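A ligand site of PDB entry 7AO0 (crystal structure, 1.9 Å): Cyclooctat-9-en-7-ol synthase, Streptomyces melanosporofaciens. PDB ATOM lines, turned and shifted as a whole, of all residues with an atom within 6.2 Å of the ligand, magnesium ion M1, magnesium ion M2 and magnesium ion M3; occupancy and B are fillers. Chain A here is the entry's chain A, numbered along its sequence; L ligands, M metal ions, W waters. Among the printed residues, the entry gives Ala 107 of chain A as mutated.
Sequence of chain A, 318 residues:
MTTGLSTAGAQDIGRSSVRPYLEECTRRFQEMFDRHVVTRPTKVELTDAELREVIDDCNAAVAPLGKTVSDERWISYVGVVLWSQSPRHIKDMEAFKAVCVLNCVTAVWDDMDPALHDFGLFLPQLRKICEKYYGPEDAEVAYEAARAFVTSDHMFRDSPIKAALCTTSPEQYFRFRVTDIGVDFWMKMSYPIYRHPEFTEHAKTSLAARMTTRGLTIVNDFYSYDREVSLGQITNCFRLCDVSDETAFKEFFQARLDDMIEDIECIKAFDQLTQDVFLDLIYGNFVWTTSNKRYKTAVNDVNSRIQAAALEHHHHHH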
ATOM      1  N   ASN A 103     -34.747 -27.453 -15.675  1.00  0.00           N
ATOM      2  CA  ASN A 103     -34.227 -26.598 -14.610  1.00  0.00           C
ATOM      3  C   ASN A 103     -32.951 -27.186 -14.023  1.00  0.00           C
ATOM      4  O   ASN A 103     -31.926 -26.495 -13.896  1.00  0.00           O
ATOM      5  CB  ASN A 103     -35.291 -26.419 -13.532  1.00  0.00           C
ATOM      6  CG  ASN A 103     -34.709 -25.952 -12.213  1.00  0.00           C
ATOM      7  OD1 ASN A 103     -34.504 -24.750 -11.997  1.00  0.00           O
ATOM      8  ND2 ASN A 103     -34.443 -26.902 -11.322  1.00  0.00           N
ATOM      9  N   THR A 106     -29.756 -27.404 -16.569  1.00  0.00           N
ATOM     10  CA  THR A 106     -29.190 -26.078 -16.812  1.00  0.00           C
ATOM     11  C   THR A 106     -28.692 -25.408 -15.548  1.00  0.00           C
ATOM     12  O   THR A 106     -27.867 -24.477 -15.642  1.00  0.00           O
ATOM     13  CB  THR A 106     -30.197 -25.164 -17.514  1.00  0.00           C
ATOM     14  OG1 THR A 106     -31.330 -24.905 -16.658  1.00  0.00           O
ATOM     15  CG2 THR A 106     -30.659 -25.787 -18.821  1.00  0.00           C
ATOM     16  N   ALA A 107     -29.145 -25.834 -14.366  1.00  0.00           N
ATOM     17  CA  ALA A 107     -28.522 -25.367 -13.128  1.00  0.00           C
ATOM     18  C   ALA A 107     -27.116 -25.932 -12.978  1.00  0.00           C
ATOM     19  O   ALA A 107     -26.218 -25.268 -12.456  1.00  0.00           O
ATOM     20  CB  ALA A 107     -29.374 -25.763 -11.920  1.00  0.00           C
ATOM     21  N   ASP A 110     -25.016 -23.859 -15.094  1.00  0.00           N
ATOM     22  CA  ASP A 110     -24.770 -22.586 -14.431  1.00  0.00           C
ATOM     23  C   ASP A 110     -23.646 -22.707 -13.416  1.00  0.00           C
ATOM     24  O   ASP A 110     -22.931 -21.744 -13.154  1.00  0.00           O
ATOM     25  CB  ASP A 110     -26.062 -22.116 -13.767  1.00  0.00           C
ATOM     26  CG  ASP A 110     -25.901 -20.830 -12.972  1.00  0.00           C
ATOM     27  OD1 ASP A 110     -25.976 -19.745 -13.596  1.00  0.00           O
ATOM     28  OD2 ASP A 110     -25.773 -20.892 -11.710  1.00  0.00           O
ATOM     29  N   ASP A 111     -23.451 -23.895 -12.855  1.00  0.00           N
ATOM     30  CA  ASP A 111     -22.402 -24.103 -11.868  1.00  0.00           C
ATOM     31  C   ASP A 111     -21.082 -24.547 -12.474  1.00  0.00           C
ATOM     32  O   ASP A 111     -20.078 -24.589 -11.764  1.00  0.00           O
ATOM     33  CB  ASP A 111     -22.865 -25.137 -10.812  1.00  0.00           C
ATOM     34  CG  ASP A 111     -23.770 -24.517  -9.771  1.00  0.00           C
ATOM     35  OD1 ASP A 111     -23.768 -23.262  -9.654  1.00  0.00           O
ATOM     36  OD2 ASP A 111     -24.494 -25.258  -9.097  1.00  0.00           O
ATOM     37  N   PHE A 149     -30.817 -19.758 -22.754  1.00  0.00           N
ATOM     38  CA  PHE A 149     -30.329 -19.608 -21.380  1.00  0.00           C
ATOM     39  C   PHE A 149     -28.890 -20.080 -21.250  1.00  0.00           C
ATOM     40  O   PHE A 149     -28.071 -19.392 -20.639  1.00  0.00           O
ATOM     41  CB  PHE A 149     -31.221 -20.379 -20.394  1.00  0.00           C
ATOM     42  CG  PHE A 149     -30.687 -20.331 -18.985  1.00  0.00           C
ATOM     43  CD1 PHE A 149     -30.844 -19.195 -18.209  1.00  0.00           C
ATOM     44  CD2 PHE A 149     -29.972 -21.417 -18.463  1.00  0.00           C
ATOM     45  CE1 PHE A 149     -30.345 -19.131 -16.906  1.00  0.00           C
ATOM     46  CE2 PHE A 149     -29.473 -21.362 -17.166  1.00  0.00           C
ATOM     47  CZ  PHE A 149     -29.649 -20.214 -16.386  1.00  0.00           C
ATOM     48  N   ASP A 153     -25.546 -17.708 -20.298  1.00  0.00           N
ATOM     49  CA  ASP A 153     -24.657 -18.004 -19.178  1.00  0.00           C
ATOM     50  C   ASP A 153     -23.207 -18.148 -19.654  1.00  0.00           C
ATOM     51  O   ASP A 153     -22.301 -17.553 -19.067  1.00  0.00           O
ATOM     52  CB  ASP A 153     -25.128 -19.283 -18.465  1.00  0.00           C
ATOM     53  CG  ASP A 153     -24.177 -19.695 -17.372  1.00  0.00           C
ATOM     54  OD1 ASP A 153     -23.900 -18.870 -16.473  1.00  0.00           O
ATOM     55  OD2 ASP A 153     -23.664 -20.827 -17.446  1.00  0.00           O
ATOM     56  N   ARG A 177     -30.859  -9.594 -15.711  1.00  0.00           N
ATOM     57  CA  ARG A 177     -31.350 -10.791 -15.029  1.00  0.00           C
ATOM     58  C   ARG A 177     -32.603 -11.401 -15.665  1.00  0.00           C
ATOM     59  O   ARG A 177     -32.869 -12.574 -15.419  1.00  0.00           O
ATOM     60  CB  ARG A 177     -31.609 -10.465 -13.558  1.00  0.00           C
ATOM     61  CG  ARG A 177     -30.299 -10.252 -12.810  1.00  0.00           C
ATOM     62  CD  ARG A 177     -29.474 -11.554 -12.785  1.00  0.00           C
ATOM     63  NE  ARG A 177     -29.413 -12.073 -11.420  1.00  0.00           N
ATOM     64  CZ  ARG A 177     -29.207 -13.344 -11.086  1.00  0.00           C
ATOM     65  NH1 ARG A 177     -29.043 -14.280 -11.999  1.00  0.00           N
ATOM     66  NH2 ARG A 177     -29.179 -13.672  -9.797  1.00  0.00           N
ATOM     67  N   ASP A 180     -30.690 -13.796 -17.535  1.00  0.00           N
ATOM     68  CA  ASP A 180     -29.620 -14.513 -16.837  1.00  0.00           C
ATOM     69  C   ASP A 180     -30.129 -15.355 -15.660  1.00  0.00           C
ATOM     70  O   ASP A 180     -29.616 -16.445 -15.417  1.00  0.00           O
ATOM     71  CB  ASP A 180     -28.561 -13.537 -16.339  1.00  0.00           C
ATOM     72  CG  ASP A 180     -27.393 -14.241 -15.668  1.00  0.00           C
ATOM     73  OD1 ASP A 180     -26.506 -14.791 -16.360  1.00  0.00           O
ATOM     74  OD2 ASP A 180     -27.342 -14.236 -14.414  1.00  0.00           O
ATOM     75  N   ILE A 181     -31.108 -14.861 -14.908  1.00  0.00           N
ATOM     76  CA  ILE A 181     -31.583 -15.678 -13.794  1.00  0.00           C
ATOM     77  C   ILE A 181     -32.391 -16.875 -14.281  1.00  0.00           C
ATOM     78  O   ILE A 181     -32.603 -17.824 -13.521  1.00  0.00           O
ATOM     79  CB  ILE A 181     -32.373 -14.859 -12.766  1.00  0.00           C
ATOM     80  CG1 ILE A 181     -32.455 -15.647 -11.456  1.00  0.00           C
ATOM     81  CG2 ILE A 181     -33.790 -14.494 -13.248  1.00  0.00           C
ATOM     82  CD1 ILE A 181     -32.744 -14.831 -10.238  1.00  0.00           C
ATOM     83  N   GLY A 182     -32.790 -16.878 -15.544  1.00  0.00           N
ATOM     84  CA  GLY A 182     -33.532 -17.991 -16.089  1.00  0.00           C
ATOM     85  C   GLY A 182     -35.039 -17.858 -16.082  1.00  0.00           C
ATOM     86  O   GLY A 182     -35.726 -18.815 -16.477  1.00  0.00           O
ATOM     87  N   ASN A 220     -33.134 -14.375  -4.445  1.00  0.00           N
ATOM     88  CA  ASN A 220     -31.983 -15.223  -4.705  1.00  0.00           C
ATOM     89  C   ASN A 220     -30.683 -14.494  -4.410  1.00  0.00           C
ATOM     90  O   ASN A 220     -29.753 -15.066  -3.832  1.00  0.00           O
ATOM     91  CB  ASN A 220     -31.984 -15.738  -6.144  1.00  0.00           C
ATOM     92  CG  ASN A 220     -30.703 -16.478  -6.435  1.00  0.00           C
ATOM     93  OD1 ASN A 220     -29.787 -15.932  -7.000  1.00  0.00           O
ATOM     94  ND2 ASN A 220     -30.615 -17.728  -5.944  1.00  0.00           N
ATOM     95  N   ASP A 221     -30.607 -13.222  -4.778  1.00  0.00           N
ATOM     96  CA  ASP A 221     -29.351 -12.519  -4.585  1.00  0.00           C
ATOM     97  C   ASP A 221     -28.993 -12.436  -3.106  1.00  0.00           C
ATOM     98  O   ASP A 221     -27.823 -12.529  -2.738  1.00  0.00           O
ATOM     99  CB  ASP A 221     -29.405 -11.125  -5.185  1.00  0.00           C
ATOM    100  CG  ASP A 221     -29.398 -11.160  -6.702  1.00  0.00           C
ATOM    101  OD1 ASP A 221     -29.224 -12.271  -7.249  1.00  0.00           O
ATOM    102  OD2 ASP A 221     -29.559 -10.085  -7.321  1.00  0.00           O
ATOM    103  N   SER A 224     -27.771 -15.934  -1.953  1.00  0.00           N
ATOM    104  CA  SER A 224     -26.617 -16.484  -2.646  1.00  0.00           C
ATOM    105  C   SER A 224     -25.418 -15.519  -2.625  1.00  0.00           C
ATOM    106  O   SER A 224     -24.359 -15.851  -3.175  1.00  0.00           O
ATOM    107  CB  SER A 224     -26.991 -16.867  -4.086  1.00  0.00           C
ATOM    108  OG  SER A 224     -27.602 -15.786  -4.796  1.00  0.00           O
ATOM    109  N   TYR A 225     -25.547 -14.367  -1.962  1.00  0.00           N
ATOM    110  CA  TYR A 225     -24.486 -13.372  -1.945  1.00  0.00           C
ATOM    111  C   TYR A 225     -23.172 -13.957  -1.411  1.00  0.00           C
ATOM    112  O   TYR A 225     -22.125 -13.866  -2.064  1.00  0.00           O
ATOM    113  CB  TYR A 225     -24.945 -12.173  -1.114  1.00  0.00           C
ATOM    114  CG  TYR A 225     -23.956 -11.051  -1.051  1.00  0.00           C
ATOM    115  CD1 TYR A 225     -22.933 -11.060  -0.106  1.00  0.00           C
ATOM    116  CD2 TYR A 225     -24.004 -10.004  -1.955  1.00  0.00           C
ATOM    117  CE1 TYR A 225     -21.998 -10.056  -0.053  1.00  0.00           C
ATOM    118  CE2 TYR A 225     -23.074  -8.978  -1.911  1.00  0.00           C
ATOM    119  CZ  TYR A 225     -22.072  -9.024  -0.937  1.00  0.00           C
ATOM    120  OH  TYR A 225     -21.142  -8.034  -0.869  1.00  0.00           O
ATOM    121  N   ARG A 227     -21.971 -17.035  -1.118  1.00  0.00           N
ATOM    122  CA  ARG A 227     -21.364 -17.983  -2.055  1.00  0.00           C
ATOM    123  C   ARG A 227     -20.824 -17.275  -3.295  1.00  0.00           C
ATOM    124  O   ARG A 227     -19.690 -17.529  -3.731  1.00  0.00           O
ATOM    125  CB  ARG A 227     -22.380 -19.050  -2.469  1.00  0.00           C
ATOM    126  CG  ARG A 227     -21.966 -19.832  -3.726  1.00  0.00           C
ATOM    127  CD  ARG A 227     -22.831 -21.066  -3.980  1.00  0.00           C
ATOM    128  NE  ARG A 227     -24.247 -20.720  -4.183  1.00  0.00           N
ATOM    129  CZ  ARG A 227     -24.749 -20.198  -5.303  1.00  0.00           C
ATOM    130  NH1 ARG A 227     -23.989 -19.953  -6.357  1.00  0.00           N
ATOM    131  NH2 ARG A 227     -26.047 -19.905  -5.381  1.00  0.00           N
ATOM    132  N   GLU A 228     -21.623 -16.385  -3.887  1.00  0.00           N
ATOM    133  CA  GLU A 228     -21.212 -15.759  -5.141  1.00  0.00           C
ATOM    134  C   GLU A 228     -19.991 -14.874  -4.939  1.00  0.00           C
ATOM    135  O   GLU A 228     -19.042 -14.944  -5.732  1.00  0.00           O
ATOM    136  CB  GLU A 228     -22.409 -14.992  -5.728  1.00  0.00           C
ATOM    137  CG  GLU A 228     -23.438 -16.000  -6.270  1.00  0.00           C
ATOM    138  CD  GLU A 228     -24.750 -15.402  -6.712  1.00  0.00           C
ATOM    139  OE1 GLU A 228     -24.943 -14.167  -6.549  1.00  0.00           O
ATOM    140  OE2 GLU A 228     -25.584 -16.195  -7.216  1.00  0.00           O
ATOM    141  N   GLN A 233     -18.156 -14.113  -8.388  1.00  0.00           N
ATOM    142  CA  GLN A 233     -19.317 -13.888  -9.259  1.00  0.00           C
ATOM    143  C   GLN A 233     -19.929 -12.510  -8.968  1.00  0.00           C
ATOM    144  O   GLN A 233     -20.211 -12.185  -7.813  1.00  0.00           O
ATOM    145  CB  GLN A 233     -20.348 -15.006  -9.063  1.00  0.00           C
ATOM    146  CG  GLN A 233     -19.813 -16.346  -9.587  1.00  0.00           C
ATOM    147  CD  GLN A 233     -20.731 -17.513  -9.303  1.00  0.00           C
ATOM    148  OE1 GLN A 233     -21.011 -17.819  -8.157  1.00  0.00           O
ATOM    149  NE2 GLN A 233     -21.204 -18.182 -10.358  1.00  0.00           N
ATOM    150  N   THR A 235     -22.760 -11.124 -10.426  1.00  0.00           N
ATOM    151  CA  THR A 235     -24.157 -10.954 -10.825  1.00  0.00           C
ATOM    152  C   THR A 235     -25.026 -11.060  -9.566  1.00  0.00           C
ATOM    153  O   THR A 235     -25.649 -12.095  -9.283  1.00  0.00           O
ATOM    154  CB  THR A 235     -24.525 -12.009 -11.877  1.00  0.00           C
ATOM    155  OG1 THR A 235     -23.595 -11.957 -12.975  1.00  0.00           O
ATOM    156  CG2 THR A 235     -25.921 -11.776 -12.424  1.00  0.00           C
ATOM    157  N   ASN A 236     -25.051  -9.981  -8.786  1.00  0.00           N
ATOM    158  CA  ASN A 236     -25.817  -9.943  -7.535  1.00  0.00           C
ATOM    159  C   ASN A 236     -26.071  -8.487  -7.177  1.00  0.00           C
ATOM    160  O   ASN A 236     -25.112  -7.715  -7.043  1.00  0.00           O
ATOM    161  CB  ASN A 236     -25.029 -10.630  -6.427  1.00  0.00           C
ATOM    162  CG  ASN A 236     -25.813 -10.752  -5.129  1.00  0.00           C
ATOM    163  OD1 ASN A 236     -26.312  -9.758  -4.578  1.00  0.00           O
ATOM    164  ND2 ASN A 236     -25.910 -11.988  -4.617  1.00  0.00           N
ATOM    165  N   ARG A 294     -27.871 -25.285  -0.224  1.00  0.00           N
ATOM    166  CA  ARG A 294     -27.038 -24.528  -1.173  1.00  0.00           C
ATOM    167  C   ARG A 294     -26.816 -23.095  -0.705  1.00  0.00           C
ATOM    168  O   ARG A 294     -25.703 -22.561  -0.805  1.00  0.00           O
ATOM    169  CB  ARG A 294     -27.682 -24.551  -2.567  1.00  0.00           C
ATOM    170  CG  ARG A 294     -27.066 -23.531  -3.563  1.00  0.00           C
ATOM    171  CD  ARG A 294     -27.758 -23.563  -4.911  1.00  0.00           C
ATOM    172  NE  ARG A 294     -27.091 -22.760  -5.939  1.00  0.00           N
ATOM    173  CZ  ARG A 294     -26.148 -23.223  -6.769  1.00  0.00           C
ATOM    174  NH1 ARG A 294     -25.746 -24.478  -6.658  1.00  0.00           N
ATOM    175  NH2 ARG A 294     -25.619 -22.434  -7.703  1.00  0.00           N
ATOM    176  N   TYR A 295     -27.848 -22.451  -0.179  1.00  0.00           N
ATOM    177  CA  TYR A 295     -27.805 -21.044   0.201  1.00  0.00           C
ATOM    178  C   TYR A 295     -27.515 -20.844   1.677  1.00  0.00           C
ATOM    179  O   TYR A 295     -28.007 -19.885   2.283  1.00  0.00           O
ATOM    180  CB  TYR A 295     -29.121 -20.367  -0.163  1.00  0.00           C
ATOM    181  CG  TYR A 295     -29.460 -20.497  -1.622  1.00  0.00           C
ATOM    182  CD1 TYR A 295     -28.561 -20.075  -2.592  1.00  0.00           C
ATOM    183  CD2 TYR A 295     -30.650 -21.061  -2.027  1.00  0.00           C
ATOM    184  CE1 TYR A 295     -28.860 -20.200  -3.955  1.00  0.00           C
ATOM    185  CE2 TYR A 295     -30.961 -21.191  -3.384  1.00  0.00           C
ATOM    186  CZ  TYR A 295     -30.063 -20.760  -4.333  1.00  0.00           C
ATOM    187  OH  TYR A 295     -30.357 -20.891  -5.659  1.00  0.00           O
HETATM  188  C1  LIG L   1     -30.303 -19.951 -11.197  1.00  0.00           C
HETATM  189  C2  LIG L   1     -30.434 -20.830 -12.447  1.00  0.00           C
HETATM  190  C3  LIG L   1     -28.935 -20.088 -10.511  1.00  0.00           C
HETATM  191  C4  LIG L   1     -28.879 -18.968  -9.483  1.00  0.00           C
HETATM  192  O1  LIG L   1     -28.492 -20.704  -7.340  1.00  0.00           O
HETATM  193  P1  LIG L   1     -27.880 -19.475  -8.026  1.00  0.00           P
HETATM  194  O2  LIG L   1     -27.777 -18.372  -6.999  1.00  0.00           O
HETATM  195  O3  LIG L   1     -26.548 -19.831  -8.581  1.00  0.00           O
HETATM  196  P2  LIG L   1     -28.096 -17.487 -10.295  1.00  0.00           P
HETATM  197  O4  LIG L   1     -26.917 -17.985 -11.096  1.00  0.00           O
HETATM  198  O5  LIG L   1     -27.613 -16.532  -9.264  1.00  0.00           O
HETATM  199  O6  LIG L   1     -29.141 -16.876 -11.209  1.00  0.00           O
HETATM  200  O7  LIG L   1     -30.180 -18.658  -9.092  1.00  0.00           O
HETATM  201  N1  LIG L   1     -31.822 -20.804 -12.910  1.00  0.00           N
HETATM  202 MG    MG M   1     -27.641 -16.294  -7.154  1.00  0.00          MG
HETATM  203 MG    MG M   2     -25.411 -19.160 -10.290  1.00  0.00          MG
HETATM  204 MG    MG M   3     -26.308 -17.842 -13.100  1.00  0.00          MG
HETATM  205  O   HOH W   1     -24.419 -17.912  -8.967  1.00  0.00           O
HETATM  206  O   HOH W   2     -26.149 -15.714 -12.857  1.00  0.00           O
HETATM  207  O   HOH W   3     -28.891 -23.208  -8.603  1.00  0.00           O
HETATM  208  O   HOH W   4     -25.720 -17.394 -15.162  1.00  0.00           O
HETATM  209  O   HOH W   5     -23.715 -20.365  -9.747  1.00  0.00           O
HETATM  210  O   HOH W   6     -28.256 -17.746 -13.580  1.00  0.00           O
HETATM  211  O   HOH W   7     -31.340 -23.404 -14.136  1.00  0.00           O
HETATM  212  O   HOH W   8     -24.424 -18.036 -12.105  1.00  0.00           O
HETATM  213  O   HOH W   9     -27.429 -14.144  -7.293  1.00  0.00           O
HETATM  214  O   HOH W  10     -25.820 -14.679 -10.116  1.00  0.00           O
HETATM  215  O   HOH W  11     -32.627 -22.931 -11.523  1.00  0.00           O
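Magnesium ion M2 is bound by water W1 (2.1 Å), O4 of the ligand (2.1 Å), water W5 (2.2 Å), O3 of the ligand (2.2 Å), OD2 of Asp 110 (2.3 Å) and water W8 (2.4 Å). Magnesium ion M2 has six donor atoms within binding distance.
Of the 22 residues printed, 3 come within 4 Å of magnesium ion M1.
Magnesium ion M3 is bound by the side-chain carboxylate (OD1) of Asp 110, water W6, an oxygen (O4) of the ligand, water W8, water W2 and water W4. Magnesium ion M3 has six donor atoms within binding distance.
Hydrophobic or aromatic side chains that line the ligand: Ile 181 and Tyr 295. Of the 22 residues printed, 9 come within 4 Å of the ligand. The nearest printed residue that does not touch the ligand is Phe 149 (4.1 Å).
O6 of the ligand is in salt-bridge range of NH1 of Arg 177 (2.7 Å). N1 of the ligand sits at hydrogen-bond distance from O of Ile 181, 3.1 Å away. An oxygen (O1) of the ligand lies within salt-bridge range of the guanidinium group of Arg 227 (3.2 Å). OH of Tyr 295 lies within hydrogen-bond range of O1 of the ligand (2.5 Å). NE of Arg 294 is in salt-bridge range of O1 of the ligand (2.9 Å).
Water W2 lies within hydrogen-bond range of the side-chain carboxylate of Asp 180 (2.5 Å) and the guanidinium group of Arg 177 (3.3 Å). Water W4 lies within hydrogen-bond range of the side-chain carboxylate of Asp 153 (2.7 Å) and the side-chain carboxylate of Asp 180 (3.0 Å). Water W6 lies within hydrogen-bond range of O of Asp 180 and O6 of the ligand. Water W11 bridges the side-chain amide oxygen (OD1) of Asn 103 (2.7 Å) and a nitrogen (N1) of the ligand (2.7 Å). Water W3 lies within hydrogen-bond range of an oxygen (O1) of the ligand (2.8 Å) and the guanidinium group (NE) of Arg 294 (3.2 Å). Water W7 lies within hydrogen-bond range of N1 of the ligand (2.9 Å), OG1 of Thr 106 (2.9 Å), O of Asn 103 (3.2 Å) and N of Ala 107 (3.3 Å).
Within 4 Å of magnesium ion M2: Asp 110. The nearest printed residue that does not touch magnesium ion M2 is Arg 294 (4.2 Å).
Merely in contact with magnesium ion M3: Asp 180 (3.97 Å).
OE2 of Glu 228 binds magnesium ion M1 (2.1 Å). O2 of the ligand is bound to magnesium ion M1. An oxygen (O5) of the ligand is bound to magnesium ion M1 (2.1 Å). Water W9 binds magnesium ion M1, 2.2 Å away. OD1 of Asn 220 is bound to magnesium ion M1. Magnesium ion M1 is bound by the side-chain hydroxyl (OG) of Ser 224. Magnesium ion M1 has six donor atoms within binding distance.
OD1 of Asp 111 lies within salt-bridge range of NH2 of Arg 294, at 2.8 Å. The backbone NH of Gln 233 sits at hydrogen-bond distance from the backbone carbonyl oxygen of Glu 228 (2.9 Å). The side-chain amide nitrogen (ND2) of Asn 220 is in hydrogen-bond range of the side-chain hydroxyl (OH) of Tyr 295, at 3.2 Å. The side-chain carboxylate (OD2) of Asp 180 lies within salt-bridge range of the guanidinium group (NH1) of Arg 177 (3.0 Å). The side-chain amide nitrogen of Asn 236 lies within hydrogen-bond range of the side-chain carboxylate of Glu 228. The guanidinium group of Arg 177 is in salt-bridge range of the side-chain carboxylate of Asp 221 (2.9 Å).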
